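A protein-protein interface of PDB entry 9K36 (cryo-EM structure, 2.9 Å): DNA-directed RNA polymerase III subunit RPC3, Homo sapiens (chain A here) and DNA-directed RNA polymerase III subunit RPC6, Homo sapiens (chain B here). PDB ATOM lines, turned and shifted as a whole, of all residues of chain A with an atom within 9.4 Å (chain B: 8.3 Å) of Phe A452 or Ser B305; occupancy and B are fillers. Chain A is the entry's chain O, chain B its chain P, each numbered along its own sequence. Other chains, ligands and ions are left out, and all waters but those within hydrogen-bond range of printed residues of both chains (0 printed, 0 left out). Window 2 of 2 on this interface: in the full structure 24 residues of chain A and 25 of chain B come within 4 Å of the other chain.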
ATOM      1  N   LEU A  11     -34.455  12.263  30.211  1.00  0.00           N
ATOM      2  CA  LEU A  11     -33.333  12.815  30.964  1.00  0.00           C
ATOM      3  C   LEU A  11     -33.537  12.647  32.465  1.00  0.00           C
ATOM      4  O   LEU A  11     -32.608  12.266  33.187  1.00  0.00           O
ATOM      5  CB  LEU A  11     -33.137  14.289  30.609  1.00  0.00           C
ATOM      6  CG  LEU A  11     -32.696  14.584  29.174  1.00  0.00           C
ATOM      7  CD1 LEU A  11     -32.545  16.083  28.962  1.00  0.00           C
ATOM      8  CD2 LEU A  11     -31.401  13.859  28.852  1.00  0.00           C
ATOM      9  N   GLU A  15     -31.201  10.366  34.899  1.00  0.00           N
ATOM     10  CA  GLU A  15     -30.437  10.977  35.979  1.00  0.00           C
ATOM     11  C   GLU A  15     -30.871  10.459  37.346  1.00  0.00           C
ATOM     12  O   GLU A  15     -30.083  10.490  38.299  1.00  0.00           O
ATOM     13  CB  GLU A  15     -30.572  12.500  35.918  1.00  0.00           C
ATOM     14  CG  GLU A  15     -29.663  13.263  36.873  1.00  0.00           C
ATOM     15  CD  GLU A  15     -28.200  13.176  36.487  1.00  0.00           C
ATOM     16  OE1 GLU A  15     -27.906  12.887  35.308  1.00  0.00           O
ATOM     17  OE2 GLU A  15     -27.341  13.395  37.367  1.00  0.00           O
ATOM     18  N   ALA A 444     -34.724  20.725  29.197  1.00  0.00           N
ATOM     19  CA  ALA A 444     -34.036  19.576  28.619  1.00  0.00           C
ATOM     20  C   ALA A 444     -32.636  19.950  28.148  1.00  0.00           C
ATOM     21  O   ALA A 444     -31.671  19.215  28.390  1.00  0.00           O
ATOM     22  CB  ALA A 444     -34.854  18.997  27.465  1.00  0.00           C
ATOM     23  N   ASN A 445     -32.501  21.103  27.484  1.00  0.00           N
ATOM     24  CA  ASN A 445     -31.192  21.545  27.018  1.00  0.00           C
ATOM     25  C   ASN A 445     -30.272  21.880  28.186  1.00  0.00           C
ATOM     26  O   ASN A 445     -29.066  21.620  28.125  1.00  0.00           O
ATOM     27  CB  ASN A 445     -31.344  22.751  26.091  1.00  0.00           C
ATOM     28  CG  ASN A 445     -32.080  22.411  24.810  1.00  0.00           C
ATOM     29  OD1 ASN A 445     -32.024  21.281  24.329  1.00  0.00           O
ATOM     30  ND2 ASN A 445     -32.772  23.395  24.246  1.00  0.00           N
ATOM     31  N   LEU A 446     -30.820  22.458  29.257  1.00  0.00           N
ATOM     32  CA  LEU A 446     -30.008  22.741  30.437  1.00  0.00           C
ATOM     33  C   LEU A 446     -29.496  21.454  31.074  1.00  0.00           C
ATOM     34  O   LEU A 446     -28.323  21.366  31.457  1.00  0.00           O
ATOM     35  CB  LEU A 446     -30.811  23.560  31.448  1.00  0.00           C
ATOM     36  CG  LEU A 446     -31.162  24.995  31.052  1.00  0.00           C
ATOM     37  CD1 LEU A 446     -31.945  25.685  32.158  1.00  0.00           C
ATOM     38  CD2 LEU A 446     -29.909  25.784  30.705  1.00  0.00           C
ATOM     39  N   ILE A 447     -30.363  20.445  31.195  1.00  0.00           N
ATOM     40  CA  ILE A 447     -29.938  19.159  31.741  1.00  0.00           C
ATOM     41  C   ILE A 447     -28.880  18.524  30.847  1.00  0.00           C
ATOM     42  O   ILE A 447     -27.896  17.954  31.333  1.00  0.00           O
ATOM     43  CB  ILE A 447     -31.154  18.230  31.931  1.00  0.00           C
ATOM     44  CG1 ILE A 447     -32.094  18.791  33.000  1.00  0.00           C
ATOM     45  CG2 ILE A 447     -30.707  16.823  32.297  1.00  0.00           C
ATOM     46  CD1 ILE A 447     -33.322  17.941  33.239  1.00  0.00           C
ATOM     47  N   GLU A 448     -29.063  18.616  29.527  1.00  0.00           N
ATOM     48  CA  GLU A 448     -28.083  18.062  28.601  1.00  0.00           C
ATOM     49  C   GLU A 448     -26.736  18.761  28.738  1.00  0.00           C
ATOM     50  O   GLU A 448     -25.687  18.110  28.725  1.00  0.00           O
ATOM     51  CB  GLU A 448     -28.599  18.167  27.165  1.00  0.00           C
ATOM     52  CG  GLU A 448     -27.647  17.609  26.116  1.00  0.00           C
ATOM     53  CD  GLU A 448     -27.480  16.104  26.217  1.00  0.00           C
ATOM     54  OE1 GLU A 448     -28.383  15.434  26.762  1.00  0.00           O
ATOM     55  OE2 GLU A 448     -26.441  15.587  25.749  1.00  0.00           O
ATOM     56  N   ARG A 449     -26.746  20.091  28.877  1.00  0.00           N
ATOM     57  CA  ARG A 449     -25.497  20.829  29.041  1.00  0.00           C
ATOM     58  C   ARG A 449     -24.814  20.473  30.354  1.00  0.00           C
ATOM     59  O   ARG A 449     -23.586  20.329  30.403  1.00  0.00           O
ATOM     60  CB  ARG A 449     -25.764  22.333  28.961  1.00  0.00           C
ATOM     61  CG  ARG A 449     -24.530  23.198  29.160  1.00  0.00           C
ATOM     62  CD  ARG A 449     -23.432  22.843  28.169  1.00  0.00           C
ATOM     63  NE  ARG A 449     -22.280  23.729  28.282  1.00  0.00           N
ATOM     64  CZ  ARG A 449     -22.127  24.849  27.583  1.00  0.00           C
ATOM     65  NH1 ARG A 449     -23.058  25.221  26.714  1.00  0.00           N
ATOM     66  NH2 ARG A 449     -21.045  25.597  27.751  1.00  0.00           N
ATOM     67  N   ARG A 450     -25.590  20.327  31.433  1.00  0.00           N
ATOM     68  CA  ARG A 450     -25.002  19.936  32.710  1.00  0.00           C
ATOM     69  C   ARG A 450     -24.373  18.551  32.624  1.00  0.00           C
ATOM     70  O   ARG A 450     -23.257  18.335  33.109  1.00  0.00           O
ATOM     71  CB  ARG A 450     -26.057  19.971  33.816  1.00  0.00           C
ATOM     72  CG  ARG A 450     -25.476  19.786  35.213  1.00  0.00           C
ATOM     73  CD  ARG A 450     -26.540  19.405  36.229  1.00  0.00           C
ATOM     74  NE  ARG A 450     -27.005  18.031  36.057  1.00  0.00           N
ATOM     75  CZ  ARG A 450     -28.132  17.693  35.439  1.00  0.00           C
ATOM     76  NH1 ARG A 450     -28.921  18.631  34.932  1.00  0.00           N
ATOM     77  NH2 ARG A 450     -28.471  16.416  35.330  1.00  0.00           N
ATOM     78  N   GLN A 451     -25.075  17.598  32.005  1.00  0.00           N
ATOM     79  CA  GLN A 451     -24.529  16.254  31.860  1.00  0.00           C
ATOM     80  C   GLN A 451     -23.290  16.252  30.973  1.00  0.00           C
ATOM     81  O   GLN A 451     -22.334  15.517  31.238  1.00  0.00           O
ATOM     82  CB  GLN A 451     -25.596  15.310  31.305  1.00  0.00           C
ATOM     83  CG  GLN A 451     -26.756  15.063  32.260  1.00  0.00           C
ATOM     84  CD  GLN A 451     -27.782  14.102  31.699  1.00  0.00           C
ATOM     85  OE1 GLN A 451     -27.638  13.601  30.584  1.00  0.00           O
ATOM     86  NE2 GLN A 451     -28.829  13.836  32.472  1.00  0.00           N
ATOM     87  N   PHE A 452     -23.281  17.083  29.927  1.00  0.00           N
ATOM     88  CA  PHE A 452     -22.107  17.176  29.065  1.00  0.00           C
ATOM     89  C   PHE A 452     -20.909  17.734  29.822  1.00  0.00           C
ATOM     90  O   PHE A 452     -19.792  17.223  29.690  1.00  0.00           O
ATOM     91  CB  PHE A 452     -22.422  18.042  27.845  1.00  0.00           C
ATOM     92  CG  PHE A 452     -21.215  18.389  27.019  1.00  0.00           C
ATOM     93  CD1 PHE A 452     -20.654  17.456  26.164  1.00  0.00           C
ATOM     94  CD2 PHE A 452     -20.650  19.652  27.091  1.00  0.00           C
ATOM     95  CE1 PHE A 452     -19.546  17.773  25.401  1.00  0.00           C
ATOM     96  CE2 PHE A 452     -19.542  19.974  26.332  1.00  0.00           C
ATOM     97  CZ  PHE A 452     -18.991  19.033  25.485  1.00  0.00           C
ATOM     98  N   GLU A 453     -21.121  18.789  30.614  1.00  0.00           N
ATOM     99  CA  GLU A 453     -20.026  19.354  31.395  1.00  0.00           C
ATOM    100  C   GLU A 453     -19.531  18.366  32.444  1.00  0.00           C
ATOM    101  O   GLU A 453     -18.329  18.305  32.733  1.00  0.00           O
ATOM    102  CB  GLU A 453     -20.464  20.662  32.055  1.00  0.00           C
ATOM    103  CG  GLU A 453     -20.617  21.821  31.087  1.00  0.00           C
ATOM    104  CD  GLU A 453     -20.765  23.155  31.793  1.00  0.00           C
ATOM    105  OE1 GLU A 453     -20.845  23.163  33.039  1.00  0.00           O
ATOM    106  OE2 GLU A 453     -20.798  24.194  31.101  1.00  0.00           O
ATOM    107  N   THR A 454     -20.442  17.588  33.030  1.00  0.00           N
ATOM    108  CA  THR A 454     -20.031  16.572  33.995  1.00  0.00           C
ATOM    109  C   THR A 454     -19.214  15.473  33.327  1.00  0.00           C
ATOM    110  O   THR A 454     -18.199  15.023  33.872  1.00  0.00           O
ATOM    111  CB  THR A 454     -21.260  15.982  34.690  1.00  0.00           C
ATOM    112  OG1 THR A 454     -22.014  17.034  35.304  1.00  0.00           O
ATOM    113  CG2 THR A 454     -20.844  14.975  35.751  1.00  0.00           C
ATOM    114  N   LYS A 455     -19.635  15.033  32.139  1.00  0.00           N
ATOM    115  CA  LYS A 455     -18.956  13.930  31.467  1.00  0.00           C
ATOM    116  C   LYS A 455     -17.596  14.359  30.921  1.00  0.00           C
ATOM    117  O   LYS A 455     -16.628  13.596  30.990  1.00  0.00           O
ATOM    118  CB  LYS A 455     -19.836  13.378  30.349  1.00  0.00           C
ATOM    119  CG  LYS A 455     -19.222  12.221  29.577  1.00  0.00           C
ATOM    120  CD  LYS A 455     -20.144  11.751  28.461  1.00  0.00           C
ATOM    121  CE  LYS A 455     -20.437  12.872  27.476  1.00  0.00           C
ATOM    122  NZ  LYS A 455     -21.364  12.434  26.393  1.00  0.00           N
ATOM    123  N   GLU A 456     -17.504  15.573  30.376  1.00  0.00           N
ATOM    124  CA  GLU A 456     -16.244  16.013  29.783  1.00  0.00           C
ATOM    125  C   GLU A 456     -15.178  16.261  30.841  1.00  0.00           C
ATOM    126  O   GLU A 456     -13.981  16.215  30.534  1.00  0.00           O
ATOM    127  CB  GLU A 456     -16.460  17.275  28.948  1.00  0.00           C
ATOM    128  CG  GLU A 456     -16.813  18.510  29.757  1.00  0.00           C
ATOM    129  CD  GLU A 456     -16.938  19.753  28.900  1.00  0.00           C
ATOM    130  OE1 GLU A 456     -16.665  19.668  27.686  1.00  0.00           O
ATOM    131  OE2 GLU A 456     -17.308  20.817  29.442  1.00  0.00           O
ATOM    132  N   ASN A 457     -15.581  16.522  32.081  1.00  0.00           N
ATOM    133  CA  ASN A 457     -14.651  16.772  33.172  1.00  0.00           C
ATOM    134  C   ASN A 457     -14.607  15.635  34.185  1.00  0.00           C
ATOM    135  O   ASN A 457     -14.122  15.835  35.302  1.00  0.00           O
ATOM    136  CB  ASN A 457     -15.002  18.086  33.874  1.00  0.00           C
ATOM    137  CG  ASN A 457     -14.941  19.277  32.943  1.00  0.00           C
ATOM    138  OD1 ASN A 457     -14.148  19.304  32.005  1.00  0.00           O
ATOM    139  ND2 ASN A 457     -15.784  20.271  33.201  1.00  0.00           N
ATOM    140  N   LYS A 458     -15.100  14.448  33.821  1.00  0.00           N
ATOM    141  CA  LYS A 458     -15.124  13.342  34.772  1.00  0.00           C
ATOM    142  C   LYS A 458     -13.720  12.872  35.133  1.00  0.00           C
ATOM    143  O   LYS A 458     -13.521  12.286  36.200  1.00  0.00           O
ATOM    144  CB  LYS A 458     -15.948  12.180  34.215  1.00  0.00           C
ATOM    145  CG  LYS A 458     -15.306  11.466  33.036  1.00  0.00           C
ATOM    146  CD  LYS A 458     -16.153  10.292  32.575  1.00  0.00           C
ATOM    147  CE  LYS A 458     -16.370   9.293  33.701  1.00  0.00           C
ATOM    148  NZ  LYS A 458     -15.083   8.772  34.236  1.00  0.00           N
ATOM    149  N   ARG A 459     -12.737  13.126  34.265  1.00  0.00           N
ATOM    150  CA  ARG A 459     -11.360  12.765  34.584  1.00  0.00           C
ATOM    151  C   ARG A 459     -10.841  13.586  35.759  1.00  0.00           C
ATOM    152  O   ARG A 459     -10.316  13.034  36.736  1.00  0.00           O
ATOM    153  CB  ARG A 459     -10.469  12.961  33.356  1.00  0.00           C
ATOM    154  CG  ARG A 459     -10.862  12.106  32.164  1.00  0.00           C
ATOM    155  CD  ARG A 459     -10.793  10.627  32.504  1.00  0.00           C
ATOM    156  NE  ARG A 459      -9.447  10.219  32.899  1.00  0.00           N
ATOM    157  CZ  ARG A 459      -9.119   8.981  33.259  1.00  0.00           C
ATOM    158  NH1 ARG A 459     -10.039   8.029  33.273  1.00  0.00           N
ATOM    159  NH2 ARG A 459      -7.869   8.700  33.605  1.00  0.00           N
ATOM    160  N   LEU A 461     -12.718  15.125  37.827  1.00  0.00           N
ATOM    161  CA  LEU A 461     -13.573  14.779  38.959  1.00  0.00           C
ATOM    162  C   LEU A 461     -13.045  13.551  39.692  1.00  0.00           C
ATOM    163  O   LEU A 461     -12.969  13.544  40.926  1.00  0.00           O
ATOM    164  CB  LEU A 461     -15.008  14.549  38.490  1.00  0.00           C
ATOM    165  CG  LEU A 461     -15.804  15.794  38.097  1.00  0.00           C
ATOM    166  CD1 LEU A 461     -17.212  15.416  37.666  1.00  0.00           C
ATOM    167  CD2 LEU A 461     -15.842  16.792  39.245  1.00  0.00           C
ATOM    168  N   LEU A 502     -16.376  24.656  36.796  1.00  0.00           N
ATOM    169  CA  LEU A 502     -17.378  23.612  36.595  1.00  0.00           C
ATOM    170  C   LEU A 502     -18.428  23.637  37.700  1.00  0.00           C
ATOM    171  O   LEU A 502     -19.627  23.495  37.433  1.00  0.00           O
ATOM    172  CB  LEU A 502     -16.703  22.243  36.529  1.00  0.00           C
ATOM    173  CG  LEU A 502     -17.635  21.032  36.476  1.00  0.00           C
ATOM    174  CD1 LEU A 502     -18.460  21.032  35.197  1.00  0.00           C
ATOM    175  CD2 LEU A 502     -16.848  19.738  36.611  1.00  0.00           C
ATOM    176  N   VAL A 506     -22.385  24.377  37.078  1.00  0.00           N
ATOM    177  CA  VAL A 506     -23.419  23.414  37.450  1.00  0.00           C
ATOM    178  C   VAL A 506     -24.423  24.048  38.405  1.00  0.00           C
ATOM    179  O   VAL A 506     -25.636  23.829  38.291  1.00  0.00           O
ATOM    180  CB  VAL A 506     -22.780  22.149  38.056  1.00  0.00           C
ATOM    181  CG1 VAL A 506     -23.845  21.249  38.665  1.00  0.00           C
ATOM    182  CG2 VAL A 506     -21.995  21.395  36.993  1.00  0.00           C
ATOM    183  N   LEU A 509     -26.668  26.363  36.368  1.00  0.00           N
ATOM    184  CA  LEU A 509     -27.575  25.574  35.541  1.00  0.00           C
ATOM    185  C   LEU A 509     -28.703  24.980  36.374  1.00  0.00           C
ATOM    186  O   LEU A 509     -29.866  24.997  35.957  1.00  0.00           O
ATOM    187  CB  LEU A 509     -26.807  24.470  34.815  1.00  0.00           C
ATOM    188  CG  LEU A 509     -25.890  24.900  33.668  1.00  0.00           C
ATOM    189  CD1 LEU A 509     -25.151  23.703  33.084  1.00  0.00           C
ATOM    190  CD2 LEU A 509     -26.683  25.620  32.592  1.00  0.00           C
ATOM    191  N   CYS B 296     -31.894  24.424  17.139  1.00  0.00           N
ATOM    192  CA  CYS B 296     -31.142  23.726  18.171  1.00  0.00           C
ATOM    193  C   CYS B 296     -31.305  22.219  18.026  1.00  0.00           C
ATOM    194  O   CYS B 296     -32.410  21.723  17.781  1.00  0.00           O
ATOM    195  CB  CYS B 296     -31.599  24.174  19.557  1.00  0.00           C
ATOM    196  SG  CYS B 296     -30.912  23.197  20.914  1.00  0.00           S
ATOM    197  N   HIS B 297     -30.202  21.489  18.178  1.00  0.00           N
ATOM    198  CA  HIS B 297     -30.228  20.037  18.115  1.00  0.00           C
ATOM    199  C   HIS B 297     -29.062  19.485  18.919  1.00  0.00           C
ATOM    200  O   HIS B 297     -28.055  20.162  19.138  1.00  0.00           O
ATOM    201  CB  HIS B 297     -30.176  19.534  16.667  1.00  0.00           C
ATOM    202  CG  HIS B 297     -30.407  18.060  16.532  1.00  0.00           C
ATOM    203  ND1 HIS B 297     -31.492  17.424  17.095  1.00  0.00           N
ATOM    204  CD2 HIS B 297     -29.692  17.099  15.901  1.00  0.00           C
ATOM    205  CE1 HIS B 297     -31.438  16.134  16.817  1.00  0.00           C
ATOM    206  NE2 HIS B 297     -30.355  15.911  16.093  1.00  0.00           N
ATOM    207  N   GLU B 298     -29.218  18.234  19.364  1.00  0.00           N
ATOM    208  CA  GLU B 298     -28.172  17.578  20.142  1.00  0.00           C
ATOM    209  C   GLU B 298     -26.901  17.405  19.319  1.00  0.00           C
ATOM    210  O   GLU B 298     -25.841  17.942  19.661  1.00  0.00           O
ATOM    211  CB  GLU B 298     -28.677  16.227  20.655  1.00  0.00           C
ATOM    212  CG  GLU B 298     -27.656  15.440  21.459  1.00  0.00           C
ATOM    213  CD  GLU B 298     -28.168  14.072  21.865  1.00  0.00           C
ATOM    214  OE1 GLU B 298     -29.309  13.728  21.497  1.00  0.00           O
ATOM    215  OE2 GLU B 298     -27.426  13.338  22.554  1.00  0.00           O
ATOM    216  N   GLY B 299     -26.991  16.653  18.224  1.00  0.00           N
ATOM    217  CA  GLY B 299     -25.850  16.441  17.358  1.00  0.00           C
ATOM    218  C   GLY B 299     -25.928  17.228  16.065  1.00  0.00           C
ATOM    219  O   GLY B 299     -26.700  16.881  15.164  1.00  0.00           O
ATOM    220  N   GLY B 300     -25.139  18.289  15.964  1.00  0.00           N
ATOM    221  CA  GLY B 300     -25.148  19.103  14.765  1.00  0.00           C
ATOM    222  C   GLY B 300     -24.235  20.297  14.921  1.00  0.00           C
ATOM    223  O   GLY B 300     -23.436  20.378  15.856  1.00  0.00           O
ATOM    224  N   GLU B 301     -24.365  21.230  13.974  1.00  0.00           N
ATOM    225  CA  GLU B 301     -23.553  22.442  14.018  1.00  0.00           C
ATOM    226  C   GLU B 301     -23.939  23.323  15.200  1.00  0.00           C
ATOM    227  O   GLU B 301     -23.071  23.905  15.860  1.00  0.00           O
ATOM    228  CB  GLU B 301     -23.696  23.213  12.706  1.00  0.00           C
ATOM    229  CG  GLU B 301     -23.336  22.406  11.466  1.00  0.00           C
ATOM    230  CD  GLU B 301     -23.502  23.204  10.190  1.00  0.00           C
ATOM    231  OE1 GLU B 301     -23.698  24.434  10.280  1.00  0.00           O
ATOM    232  OE2 GLU B 301     -23.441  22.603   9.096  1.00  0.00           O
ATOM    233  N   ILE B 302     -25.234  23.429  15.486  1.00  0.00           N
ATOM    234  CA  ILE B 302     -25.741  24.232  16.591  1.00  0.00           C
ATOM    235  C   ILE B 302     -26.117  23.265  17.705  1.00  0.00           C
ATOM    236  O   ILE B 302     -27.193  22.659  17.687  1.00  0.00           O
ATOM    237  CB  ILE B 302     -26.932  25.102  16.173  1.00  0.00           C
ATOM    238  CG1 ILE B 302     -26.538  26.014  15.010  1.00  0.00           C
ATOM    239  CG2 ILE B 302     -27.434  25.925  17.353  1.00  0.00           C
ATOM    240  CD1 ILE B 302     -27.661  26.893  14.509  1.00  0.00           C
ATOM    241  N   SER B 303     -25.228  23.114  18.681  1.00  0.00           N
ATOM    242  CA  SER B 303     -25.420  22.201  19.794  1.00  0.00           C
ATOM    243  C   SER B 303     -25.203  22.935  21.109  1.00  0.00           C
ATOM    244  O   SER B 303     -24.401  23.872  21.177  1.00  0.00           O
ATOM    245  CB  SER B 303     -24.455  21.012  19.702  1.00  0.00           C
ATOM    246  OG  SER B 303     -24.616  20.123  20.794  1.00  0.00           O
ATOM    247  N   PRO B 304     -25.919  22.541  22.165  1.00  0.00           N
ATOM    248  CA  PRO B 304     -25.680  23.164  23.477  1.00  0.00           C
ATOM    249  C   PRO B 304     -24.273  22.942  24.005  1.00  0.00           C
ATOM    250  O   PRO B 304     -23.786  23.755  24.801  1.00  0.00           O
ATOM    251  CB  PRO B 304     -26.735  22.505  24.378  1.00  0.00           C
ATOM    252  CG  PRO B 304     -27.129  21.250  23.663  1.00  0.00           C
ATOM    253  CD  PRO B 304     -27.030  21.577  22.207  1.00  0.00           C
ATOM    254  N   SER B 305     -23.605  21.865  23.587  1.00  0.00           N
ATOM    255  CA  SER B 305     -22.249  21.607  24.063  1.00  0.00           C
ATOM    256  C   SER B 305     -21.273  22.666  23.566  1.00  0.00           C
ATOM    257  O   SER B 305     -20.421  23.142  24.324  1.00  0.00           O
ATOM    258  CB  SER B 305     -21.799  20.215  23.627  1.00  0.00           C
ATOM    259  OG  SER B 305     -21.864  20.077  22.220  1.00  0.00           O
ATOM    260  N   ASN B 306     -21.382  23.051  22.293  1.00  0.00           N
ATOM    261  CA  ASN B 306     -20.496  24.044  21.701  1.00  0.00           C
ATOM    262  C   ASN B 306     -21.191  25.381  21.463  1.00  0.00           C
ATOM    263  O   ASN B 306     -20.855  26.093  20.512  1.00  0.00           O
ATOM    264  CB  ASN B 306     -19.900  23.512  20.394  1.00  0.00           C
ATOM    265  CG  ASN B 306     -20.951  22.957  19.449  1.00  0.00           C
ATOM    266  OD1 ASN B 306     -22.126  23.323  19.520  1.00  0.00           O
ATOM    267  ND2 ASN B 306     -20.532  22.066  18.560  1.00  0.00           N
ATOM    268  N   CYS B 307     -22.152  25.735  22.313  1.00  0.00           N
ATOM    269  CA  CYS B 307     -22.882  26.986  22.143  1.00  0.00           C
ATOM    270  C   CYS B 307     -22.001  28.174  22.504  1.00  0.00           C
ATOM    271  O   CYS B 307     -21.248  28.132  23.482  1.00  0.00           O
ATOM    272  CB  CYS B 307     -24.141  26.981  23.003  1.00  0.00           C
ATOM    273  SG  CYS B 307     -24.983  28.578  23.085  1.00  0.00           S
ATOM    274  N   ILE B 308     -22.095  29.240  21.708  1.00  0.00           N
ATOM    275  CA  ILE B 308     -21.328  30.449  21.995  1.00  0.00           C
ATOM    276  C   ILE B 308     -22.067  31.323  23.003  1.00  0.00           C
ATOM    277  O   ILE B 308     -21.447  31.985  23.844  1.00  0.00           O
ATOM    278  CB  ILE B 308     -21.029  31.210  20.689  1.00  0.00           C
ATOM    279  CG1 ILE B 308     -20.307  30.299  19.693  1.00  0.00           C
ATOM    280  CG2 ILE B 308     -20.199  32.455  20.969  1.00  0.00           C
ATOM    281  CD1 ILE B 308     -18.972  29.779  20.187  1.00  0.00           C
ATOM    282  N   MET B 310     -24.113  30.425  25.594  1.00  0.00           N
ATOM    283  CA  MET B 310     -23.887  29.946  26.952  1.00  0.00           C
ATOM    284  C   MET B 310     -22.423  30.070  27.357  1.00  0.00           C
ATOM    285  O   MET B 310     -22.130  30.288  28.534  1.00  0.00           O
ATOM    286  CB  MET B 310     -24.367  28.502  27.090  1.00  0.00           C
ATOM    287  CG  MET B 310     -25.879  28.370  27.095  1.00  0.00           C
ATOM    288  SD  MET B 310     -26.441  26.702  27.467  1.00  0.00           S
ATOM    289  CE  MET B 310     -25.859  25.831  26.017  1.00  0.00           C
ATOM    290  N   THR B 311     -21.499  29.957  26.399  1.00  0.00           N
ATOM    291  CA  THR B 311     -20.086  30.147  26.713  1.00  0.00           C
ATOM    292  C   THR B 311     -19.821  31.566  27.206  1.00  0.00           C
ATOM    293  O   THR B 311     -19.198  31.767  28.254  1.00  0.00           O
ATOM    294  CB  THR B 311     -19.227  29.835  25.488  1.00  0.00           C
ATOM    295  OG1 THR B 311     -19.451  28.480  25.080  1.00  0.00           O
ATOM    296  CG2 THR B 311     -17.752  30.027  25.812  1.00  0.00           C
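Of the 22 printed residues of chain A, 3 touch a printed residue of chain B. Hydrophobic or aromatic side chains of chain A within 4 Å of the printed part of chain B: Phe A452. Of the 15 printed residues of chain B, 4 touch a printed residue of chain A. Hydrophobic or aromatic side chains of chain B within 4 Å of the printed part of chain A: Met B310. Among the printed residues, no Asp or Glu carboxylate lies within 4 Å of a Lys or Arg side-chain nitrogen of the other chain.
NH1 of Arg A449 is in hydrogen-bond range of O of Pro B304 (2.5 Å). The guanidinium group (NH1) of Arg A449 sits close to the side-chain sulfur (SD) of Met B310 (3.8 Å).
The guanidinium group (NE) of Arg A449 lies within salt-bridge range of the side-chain carboxylate (OE2) of Glu A453, 3.2 Å away. OG of Ser B303 is in hydrogen-bond range of OG of Ser B305 (3.1 Å). SG of Cys B307 lies within hydrogen-bond range of N of Met B310 (3.2 Å).
Printed residues of chain B within 4 Å of Asn A445: Cys B296. Of the printed residues of chain B, Arg A449 touches Pro B304 (2.5 Å) and Met B310 (3.0 Å). Phe A452 touches just one residue of chain B: Ser B305 (3.5 Å). Asn A457 touches none of the printed residues of chain B. Lys A458 touches none of the printed residues of chain B. Printed residues of chain A within 4 Å of Cys B296: Asn A445 (3.8 Å). No residue of chain A comes within 4 Å of Ser B303. Ser B305 touches just one residue of chain A: Phe A452 (3.5 Å). Printed residues of chain A within 4 Å of Met B310: Arg A449 (3.0 Å). The nearest residue of chain B that does not touch Phe A452 is Asn B306 (5.4 Å). The nearest residue of chain A that does not touch Ser B305 is Arg A449 (4.1 Å). The nearest printed residue of chain A that does not touch Cys B296 is Ala A444 (8.1 Å).
ND2 of Asn A445 touches SG of Cys B296 (3.8 Å). CE2 of Phe A452 touches CB of Ser B305 (3.5 Å).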
